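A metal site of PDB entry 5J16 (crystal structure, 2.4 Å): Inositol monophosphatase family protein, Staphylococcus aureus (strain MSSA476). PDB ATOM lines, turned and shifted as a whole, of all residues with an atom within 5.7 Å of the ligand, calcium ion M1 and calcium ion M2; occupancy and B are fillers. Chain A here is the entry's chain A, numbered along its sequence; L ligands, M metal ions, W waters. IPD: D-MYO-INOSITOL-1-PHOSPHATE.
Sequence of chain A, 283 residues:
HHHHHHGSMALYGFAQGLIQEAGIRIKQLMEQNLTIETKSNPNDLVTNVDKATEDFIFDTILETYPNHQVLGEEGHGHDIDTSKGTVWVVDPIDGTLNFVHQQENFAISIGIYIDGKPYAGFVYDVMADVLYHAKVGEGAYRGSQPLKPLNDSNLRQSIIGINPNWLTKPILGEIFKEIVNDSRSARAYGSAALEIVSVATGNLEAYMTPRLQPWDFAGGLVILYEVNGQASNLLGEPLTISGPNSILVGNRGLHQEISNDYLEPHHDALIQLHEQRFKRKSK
Asp 50 touches calcium ion M2.
Of the 23 residues printed, 4 come within 4 Å of calcium ion M2.
The nearest printed residue that does not touch calcium ion M2 is Glu 74 (4.1 Å).
Residues that only touch the ligand: Arg 211 (3.7 Å) and Leu 212 (3.8 Å).
Hydrophobic or aromatic side chains within 4 Å of the ligand: Ala 192 and Leu 212.
12 residues have an atom within 4 Å of the ligand: Glu 73, Asp 91, Ile 93, Asp 94, Gly 95, Thr 96, Gly 190, Ser 191, Ala 192, Arg 211, Leu 212 and Asp 216.
Water W2 lies within hydrogen-bond range of NE1 of Trp 215 and OD1 of Asp 216.
Water W1 lies within hydrogen-bond range of an oxygen (O8) of the ligand (2.9 Å) and the backbone NH of Leu 97 (3.4 Å).
The backbone NH of Gly 95 is in hydrogen-bond range of an oxygen (O8) of the ligand (2.7 Å).
The backbone NH of Thr 96 is in hydrogen-bond range of an oxygen (O8) of the ligand, 2.7 Å away.
O8 of the ligand lies within hydrogen-bond range of OG1 of Thr 96 (3.2 Å).
The backbone carbonyl oxygen (O) of Gly 190 lies close to an oxygen (O3) of the ligand.
O2 of the ligand lies within hydrogen-bond range of N of Ala 192 (3.2 Å).
N of Ser 191 sits at hydrogen-bond distance from O3 of the ligand.
Within 4 Å of calcium ion M1: Glu 73, Asp 91, Asp 94 and Asp 216.
The nearest printed residue that does not touch calcium ion M1 is Trp 215 (4.5 Å).
Calcium ion M2 is bound by OE1 of Glu 73 (2.2 Å), O9 of the ligand (2.4 Å), OD1 of Asp 91 (2.4 Å) and O of Ile 93 (2.5 Å).
The backbone NH (N) of Ala 192 lies within hydrogen-bond range of the side-chain carboxylate (OD2) of Asp 94, 3.2 Å away.
OG of Ser 191 is in hydrogen-bond range of OD2 of Asp 94 (2.9 Å).
OD2 of Asp 94 is in hydrogen-bond range of N of Ala 193.
N of Gly 190 sits at hydrogen-bond distance from OE1 of Glu 195 (3.4 Å).
N of Ser 191 sits at hydrogen-bond distance from OE1 of Glu 195, at 3.3 Å.
Calcium ion M1 is bound by OD2 of Asp 216 (2.1 Å), OD2 of Asp 91 (2.2 Å), O9 of the ligand (2.3 Å), OD1 of Asp 94 (2.4 Å), O1 of the ligand (2.4 Å) and water W2 (2.4 Å).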
ATOM      1  N   ASP A  50     -20.665 -21.159  14.637  1.00  0.00           N
ATOM      2  CA  ASP A  50     -21.794 -21.195  13.686  1.00  0.00           C
ATOM      3  C   ASP A  50     -23.099 -20.884  14.433  1.00  0.00           C
ATOM      4  O   ASP A  50     -23.943 -20.151  13.924  1.00  0.00           O
ATOM      5  CB  ASP A  50     -22.010 -22.570  13.024  1.00  0.00           C
ATOM      6  CG  ASP A  50     -20.822 -23.050  12.254  1.00  0.00           C
ATOM      7  OD1 ASP A  50     -20.975 -23.265  11.042  1.00  0.00           O
ATOM      8  OD2 ASP A  50     -19.765 -23.250  12.877  1.00  0.00           O
ATOM      9  N   GLU A  73     -29.365 -23.481   8.834  1.00  0.00           N
ATOM     10  CA  GLU A  73     -28.783 -24.827   8.912  1.00  0.00           C
ATOM     11  C   GLU A  73     -28.682 -25.334  10.326  1.00  0.00           C
ATOM     12  O   GLU A  73     -29.138 -26.440  10.622  1.00  0.00           O
ATOM     13  CB  GLU A  73     -27.459 -24.952   8.135  1.00  0.00           C
ATOM     14  CG  GLU A  73     -26.120 -24.879   8.867  1.00  0.00           C
ATOM     15  CD  GLU A  73     -25.145 -25.878   8.292  1.00  0.00           C
ATOM     16  OE1 GLU A  73     -24.190 -25.435   7.622  1.00  0.00           O
ATOM     17  OE2 GLU A  73     -25.364 -27.096   8.484  1.00  0.00           O
ATOM     18  N   GLU A  74     -28.137 -24.496  11.215  1.00  0.00           N
ATOM     19  CA  GLU A  74     -27.970 -24.835  12.647  1.00  0.00           C
ATOM     20  C   GLU A  74     -29.293 -24.705  13.438  1.00  0.00           C
ATOM     21  O   GLU A  74     -29.282 -24.361  14.628  1.00  0.00           O
ATOM     22  CB  GLU A  74     -26.801 -24.034  13.295  1.00  0.00           C
ATOM     23  CG  GLU A  74     -25.532 -24.848  13.531  1.00  0.00           C
ATOM     24  CD  GLU A  74     -24.760 -25.173  12.253  1.00  0.00           C
ATOM     25  OE1 GLU A  74     -24.500 -24.255  11.456  1.00  0.00           O
ATOM     26  OE2 GLU A  74     -24.394 -26.355  12.069  1.00  0.00           O
ATOM     27  N   ASP A  91     -26.968 -19.458   5.861  1.00  0.00           N
ATOM     28  CA  ASP A  91     -25.868 -20.308   6.244  1.00  0.00           C
ATOM     29  C   ASP A  91     -24.924 -19.331   6.894  1.00  0.00           C
ATOM     30  O   ASP A  91     -24.408 -18.452   6.228  1.00  0.00           O
ATOM     31  CB  ASP A  91     -25.227 -20.956   4.999  1.00  0.00           C
ATOM     32  CG  ASP A  91     -24.326 -22.119   5.337  1.00  0.00           C
ATOM     33  OD1 ASP A  91     -23.920 -22.237   6.497  1.00  0.00           O
ATOM     34  OD2 ASP A  91     -24.000 -22.887   4.388  1.00  0.00           O
ATOM     35  N   PRO A  92     -24.769 -19.427   8.218  1.00  0.00           N
ATOM     36  CA  PRO A  92     -23.891 -18.476   8.928  1.00  0.00           C
ATOM     37  C   PRO A  92     -22.398 -18.652   8.629  1.00  0.00           C
ATOM     38  O   PRO A  92     -21.690 -17.666   8.660  1.00  0.00           O
ATOM     39  CB  PRO A  92     -24.193 -18.772  10.399  1.00  0.00           C
ATOM     40  CG  PRO A  92     -24.673 -20.181  10.407  1.00  0.00           C
ATOM     41  CD  PRO A  92     -25.499 -20.299   9.153  1.00  0.00           C
ATOM     42  N   ILE A  93     -21.915 -19.873   8.394  1.00  0.00           N
ATOM     43  CA  ILE A  93     -20.540 -20.103   7.902  1.00  0.00           C
ATOM     44  C   ILE A  93     -20.612 -21.228   6.876  1.00  0.00           C
ATOM     45  O   ILE A  93     -20.733 -22.388   7.260  1.00  0.00           O
ATOM     46  CB  ILE A  93     -19.502 -20.527   9.016  1.00  0.00           C
ATOM     47  CG1 ILE A  93     -19.125 -19.331   9.919  1.00  0.00           C
ATOM     48  CG2 ILE A  93     -18.200 -21.045   8.401  1.00  0.00           C
ATOM     49  CD1 ILE A  93     -19.915 -19.260  11.211  1.00  0.00           C
ATOM     50  N   ASP A  94     -20.564 -20.862   5.589  1.00  0.00           N
ATOM     51  CA  ASP A  94     -20.418 -21.819   4.528  1.00  0.00           C
ATOM     52  C   ASP A  94     -18.936 -22.005   4.311  1.00  0.00           C
ATOM     53  O   ASP A  94     -18.243 -21.065   4.040  1.00  0.00           O
ATOM     54  CB  ASP A  94     -21.125 -21.367   3.255  1.00  0.00           C
ATOM     55  CG  ASP A  94     -21.176 -22.489   2.188  1.00  0.00           C
ATOM     56  OD1 ASP A  94     -21.607 -23.627   2.527  1.00  0.00           O
ATOM     57  OD2 ASP A  94     -20.744 -22.249   1.040  1.00  0.00           O
ATOM     58  N   GLY A  95     -18.513 -23.260   4.361  1.00  0.00           N
ATOM     59  CA  GLY A  95     -17.123 -23.628   4.376  1.00  0.00           C
ATOM     60  C   GLY A  95     -16.552 -23.714   5.767  1.00  0.00           C
ATOM     61  O   GLY A  95     -15.525 -23.073   6.037  1.00  0.00           O
ATOM     62  N   THR A  96     -17.175 -24.484   6.653  1.00  0.00           N
ATOM     63  CA  THR A  96     -16.614 -24.635   8.017  1.00  0.00           C
ATOM     64  C   THR A  96     -15.269 -25.360   8.068  1.00  0.00           C
ATOM     65  O   THR A  96     -14.452 -25.062   8.919  1.00  0.00           O
ATOM     66  CB  THR A  96     -17.557 -25.308   9.050  1.00  0.00           C
ATOM     67  OG1 THR A  96     -18.428 -26.215   8.390  1.00  0.00           O
ATOM     68  CG2 THR A  96     -18.397 -24.279   9.743  1.00  0.00           C
ATOM     69  N   LEU A  97     -15.042 -26.309   7.167  1.00  0.00           N
ATOM     70  CA  LEU A  97     -13.736 -26.966   7.092  1.00  0.00           C
ATOM     71  C   LEU A  97     -12.693 -25.934   6.710  1.00  0.00           C
ATOM     72  O   LEU A  97     -11.665 -25.851   7.348  1.00  0.00           O
ATOM     73  CB  LEU A  97     -13.750 -28.107   6.085  1.00  0.00           C
ATOM     74  CG  LEU A  97     -14.305 -29.376   6.676  1.00  0.00           C
ATOM     75  CD1 LEU A  97     -14.688 -30.360   5.555  1.00  0.00           C
ATOM     76  CD2 LEU A  97     -13.288 -30.008   7.639  1.00  0.00           C
ATOM     77  N   TRP A 166     -16.708 -36.587  -5.133  1.00  0.00           N
ATOM     78  CA  TRP A 166     -17.816 -37.067  -5.971  1.00  0.00           C
ATOM     79  C   TRP A 166     -17.389 -38.102  -6.999  1.00  0.00           C
ATOM     80  O   TRP A 166     -18.214 -38.885  -7.421  1.00  0.00           O
ATOM     81  CB  TRP A 166     -18.602 -35.903  -6.668  1.00  0.00           C
ATOM     82  CG  TRP A 166     -18.971 -34.886  -5.696  1.00  0.00           C
ATOM     83  CD1 TRP A 166     -18.712 -33.538  -5.768  1.00  0.00           C
ATOM     84  CD2 TRP A 166     -19.564 -35.114  -4.414  1.00  0.00           C
ATOM     85  NE1 TRP A 166     -19.152 -32.907  -4.633  1.00  0.00           N
ATOM     86  CE2 TRP A 166     -19.670 -33.854  -3.779  1.00  0.00           C
ATOM     87  CE3 TRP A 166     -20.049 -36.253  -3.766  1.00  0.00           C
ATOM     88  CZ2 TRP A 166     -20.264 -33.692  -2.512  1.00  0.00           C
ATOM     89  CZ3 TRP A 166     -20.625 -36.104  -2.502  1.00  0.00           C
ATOM     90  CH2 TRP A 166     -20.737 -34.822  -1.891  1.00  0.00           C
ATOM     91  N   TYR A 189     -12.890 -25.585  -4.188  1.00  0.00           N
ATOM     92  CA  TYR A 189     -12.578 -24.547  -3.224  1.00  0.00           C
ATOM     93  C   TYR A 189     -13.161 -24.828  -1.844  1.00  0.00           C
ATOM     94  O   TYR A 189     -12.722 -24.221  -0.862  1.00  0.00           O
ATOM     95  CB  TYR A 189     -13.020 -23.176  -3.780  1.00  0.00           C
ATOM     96  CG  TYR A 189     -12.348 -22.839  -5.141  1.00  0.00           C
ATOM     97  CD1 TYR A 189     -10.969 -22.895  -5.292  1.00  0.00           C
ATOM     98  CD2 TYR A 189     -13.094 -22.431  -6.241  1.00  0.00           C
ATOM     99  CE1 TYR A 189     -10.352 -22.574  -6.491  1.00  0.00           C
ATOM    100  CE2 TYR A 189     -12.497 -22.107  -7.440  1.00  0.00           C
ATOM    101  CZ  TYR A 189     -11.122 -22.188  -7.558  1.00  0.00           C
ATOM    102  OH  TYR A 189     -10.496 -21.872  -8.748  1.00  0.00           O
ATOM    103  N   GLY A 190     -14.093 -25.751  -1.735  1.00  0.00           N
ATOM    104  CA  GLY A 190     -14.668 -26.052  -0.416  1.00  0.00           C
ATOM    105  C   GLY A 190     -15.659 -25.034   0.122  1.00  0.00           C
ATOM    106  O   GLY A 190     -15.873 -24.965   1.368  1.00  0.00           O
ATOM    107  N   SER A 191     -16.291 -24.262  -0.767  1.00  0.00           N
ATOM    108  CA  SER A 191     -17.466 -23.458  -0.384  1.00  0.00           C
ATOM    109  C   SER A 191     -18.451 -23.416  -1.520  1.00  0.00           C
ATOM    110  O   SER A 191     -18.182 -22.784  -2.553  1.00  0.00           O
ATOM    111  CB  SER A 191     -17.108 -22.022   0.031  1.00  0.00           C
ATOM    112  OG  SER A 191     -18.264 -21.180   0.107  1.00  0.00           O
ATOM    113  N   ALA A 192     -19.582 -24.050  -1.351  1.00  0.00           N
ATOM    114  CA  ALA A 192     -20.581 -24.029  -2.378  1.00  0.00           C
ATOM    115  C   ALA A 192     -21.063 -22.580  -2.688  1.00  0.00           C
ATOM    116  O   ALA A 192     -21.225 -22.190  -3.851  1.00  0.00           O
ATOM    117  CB  ALA A 192     -21.743 -24.919  -1.980  1.00  0.00           C
ATOM    118  N   ALA A 193     -21.285 -21.789  -1.647  1.00  0.00           N
ATOM    119  CA  ALA A 193     -21.740 -20.419  -1.857  1.00  0.00           C
ATOM    120  C   ALA A 193     -20.733 -19.640  -2.669  1.00  0.00           C
ATOM    121  O   ALA A 193     -21.131 -19.000  -3.638  1.00  0.00           O
ATOM    122  CB  ALA A 193     -21.989 -19.718  -0.540  1.00  0.00           C
ATOM    123  N   GLU A 195     -18.256 -20.889  -4.600  1.00  0.00           N
ATOM    124  CA  GLU A 195     -18.200 -21.466  -5.935  1.00  0.00           C
ATOM    125  C   GLU A 195     -19.320 -21.109  -6.887  1.00  0.00           C
ATOM    126  O   GLU A 195     -19.099 -20.999  -8.093  1.00  0.00           O
ATOM    127  CB  GLU A 195     -18.038 -22.973  -5.844  1.00  0.00           C
ATOM    128  CG  GLU A 195     -16.621 -23.274  -5.421  1.00  0.00           C
ATOM    129  CD  GLU A 195     -16.397 -24.691  -5.148  1.00  0.00           C
ATOM    130  OE1 GLU A 195     -16.590 -25.084  -3.980  1.00  0.00           O
ATOM    131  OE2 GLU A 195     -16.039 -25.387  -6.098  1.00  0.00           O
ATOM    132  N   TYR A 207     -20.175 -25.278 -12.076  1.00  0.00           N
ATOM    133  CA  TYR A 207     -19.950 -25.908 -10.780  1.00  0.00           C
ATOM    134  C   TYR A 207     -21.021 -26.934 -10.560  1.00  0.00           C
ATOM    135  O   TYR A 207     -22.142 -26.753 -11.011  1.00  0.00           O
ATOM    136  CB  TYR A 207     -20.003 -24.867  -9.667  1.00  0.00           C
ATOM    137  CG  TYR A 207     -20.252 -25.416  -8.264  1.00  0.00           C
ATOM    138  CD1 TYR A 207     -19.330 -26.219  -7.615  1.00  0.00           C
ATOM    139  CD2 TYR A 207     -21.414 -25.100  -7.581  1.00  0.00           C
ATOM    140  CE1 TYR A 207     -19.558 -26.702  -6.324  1.00  0.00           C
ATOM    141  CE2 TYR A 207     -21.651 -25.574  -6.308  1.00  0.00           C
ATOM    142  CZ  TYR A 207     -20.728 -26.374  -5.669  1.00  0.00           C
ATOM    143  OH  TYR A 207     -21.009 -26.804  -4.382  1.00  0.00           O
ATOM    144  N   THR A 209     -22.624 -30.492  -7.991  1.00  0.00           N
ATOM    145  CA  THR A 209     -22.576 -31.291  -6.776  1.00  0.00           C
ATOM    146  C   THR A 209     -23.890 -32.064  -6.655  1.00  0.00           C
ATOM    147  O   THR A 209     -24.927 -31.595  -7.091  1.00  0.00           O
ATOM    148  CB  THR A 209     -22.268 -30.394  -5.523  1.00  0.00           C
ATOM    149  OG1 THR A 209     -22.386 -31.155  -4.315  1.00  0.00           O
ATOM    150  CG2 THR A 209     -23.195 -29.242  -5.435  1.00  0.00           C
ATOM    151  N   ARG A 211     -25.342 -33.029  -3.668  1.00  0.00           N
ATOM    152  CA  ARG A 211     -26.128 -32.609  -2.504  1.00  0.00           C
ATOM    153  C   ARG A 211     -25.773 -31.188  -1.976  1.00  0.00           C
ATOM    154  O   ARG A 211     -24.688 -30.945  -1.453  1.00  0.00           O
ATOM    155  CB  ARG A 211     -26.001 -33.621  -1.360  1.00  0.00           C
ATOM    156  CG  ARG A 211     -26.991 -33.345  -0.226  1.00  0.00           C
ATOM    157  CD  ARG A 211     -27.193 -34.457   0.833  1.00  0.00           C
ATOM    158  NE  ARG A 211     -28.517 -34.278   1.481  1.00  0.00           N
ATOM    159  CZ  ARG A 211     -29.646 -34.928   1.189  1.00  0.00           C
ATOM    160  NH1 ARG A 211     -29.676 -35.905   0.292  1.00  0.00           N
ATOM    161  NH2 ARG A 211     -30.778 -34.620   1.828  1.00  0.00           N
ATOM    162  N   LEU A 212     -26.727 -30.292  -2.102  1.00  0.00           N
ATOM    163  CA  LEU A 212     -26.755 -29.050  -1.371  1.00  0.00           C
ATOM    164  C   LEU A 212     -28.070 -28.802  -0.629  1.00  0.00           C
ATOM    165  O   LEU A 212     -29.128 -29.264  -1.056  1.00  0.00           O
ATOM    166  CB  LEU A 212     -26.515 -27.944  -2.376  1.00  0.00           C
ATOM    167  CG  LEU A 212     -25.249 -27.136  -2.226  1.00  0.00           C
ATOM    168  CD1 LEU A 212     -24.003 -27.892  -1.805  1.00  0.00           C
ATOM    169  CD2 LEU A 212     -25.017 -26.302  -3.492  1.00  0.00           C
ATOM    170  N   TRP A 215     -29.932 -23.372   2.150  1.00  0.00           N
ATOM    171  CA  TRP A 215     -29.046 -22.310   2.722  1.00  0.00           C
ATOM    172  C   TRP A 215     -27.691 -22.164   1.992  1.00  0.00           C
ATOM    173  O   TRP A 215     -27.071 -21.091   2.030  1.00  0.00           O
ATOM    174  CB  TRP A 215     -28.852 -22.470   4.240  1.00  0.00           C
ATOM    175  CG  TRP A 215     -28.607 -23.874   4.736  1.00  0.00           C
ATOM    176  CD1 TRP A 215     -27.413 -24.527   4.772  1.00  0.00           C
ATOM    177  CD2 TRP A 215     -29.584 -24.799   5.231  1.00  0.00           C
ATOM    178  NE1 TRP A 215     -27.584 -25.805   5.246  1.00  0.00           N
ATOM    179  CE2 TRP A 215     -28.901 -25.997   5.549  1.00  0.00           C
ATOM    180  CE3 TRP A 215     -30.983 -24.742   5.413  1.00  0.00           C
ATOM    181  CZ2 TRP A 215     -29.568 -27.144   6.073  1.00  0.00           C
ATOM    182  CZ3 TRP A 215     -31.657 -25.867   5.912  1.00  0.00           C
ATOM    183  CH2 TRP A 215     -30.941 -27.052   6.239  1.00  0.00           C
ATOM    184  N   ASP A 216     -27.240 -23.222   1.323  1.00  0.00           N
ATOM    185  CA  ASP A 216     -25.972 -23.182   0.565  1.00  0.00           C
ATOM    186  C   ASP A 216     -26.107 -22.428  -0.772  1.00  0.00           C
ATOM    187  O   ASP A 216     -25.133 -21.847  -1.255  1.00  0.00           O
ATOM    188  CB  ASP A 216     -25.420 -24.609   0.273  1.00  0.00           C
ATOM    189  CG  ASP A 216     -25.027 -25.398   1.549  1.00  0.00           C
ATOM    190  OD1 ASP A 216     -25.342 -26.652   1.600  1.00  0.00           O
ATOM    191  OD2 ASP A 216     -24.407 -24.796   2.477  1.00  0.00           O
HETATM  192  C1  IPD L   1     -20.579 -27.306   2.976  1.00  0.00           C
HETATM  193  C2  IPD L   1     -19.783 -26.472   1.977  1.00  0.00           C
HETATM  194  C3  IPD L   1     -18.938 -27.475   1.142  1.00  0.00           C
HETATM  195  C4  IPD L   1     -19.816 -28.428   0.334  1.00  0.00           C
HETATM  196  C5  IPD L   1     -20.774 -29.212   1.244  1.00  0.00           C
HETATM  197  C6  IPD L   1     -21.565 -28.239   2.211  1.00  0.00           C
HETATM  198  P1  IPD L   1     -20.747 -26.206   5.457  1.00  0.00           P
HETATM  199  O1  IPD L   1     -21.284 -26.508   3.910  1.00  0.00           O
HETATM  200  O2  IPD L   1     -20.678 -25.697   1.124  1.00  0.00           O
HETATM  201  O3  IPD L   1     -18.033 -26.839   0.265  1.00  0.00           O
HETATM  202  O4  IPD L   1     -19.007 -29.391  -0.270  1.00  0.00           O
HETATM  203  O5  IPD L   1     -21.655 -29.925   0.361  1.00  0.00           O
HETATM  204  O6  IPD L   1     -22.268 -29.001   3.160  1.00  0.00           O
HETATM  205  O7  IPD L   1     -20.823 -27.368   6.406  1.00  0.00           O
HETATM  206  O8  IPD L   1     -19.208 -25.683   5.304  1.00  0.00           O
HETATM  207  O9  IPD L   1     -21.655 -24.912   5.907  1.00  0.00           O
HETATM  208 CA    CA M   1     -22.999 -24.819   4.019  1.00  0.00          CA
HETATM  209 CA    CA M   2     -22.674 -23.859   7.810  1.00  0.00          CA
HETATM  210  O   HOH W   1     -16.939 -27.358   4.570  1.00  0.00           O
HETATM  211  O   HOH W   2     -24.588 -26.415   4.900  1.00  0.00           O
HETATM  212  O   HOH W   3     -16.369 -29.077  -0.212  1.00  0.00           O
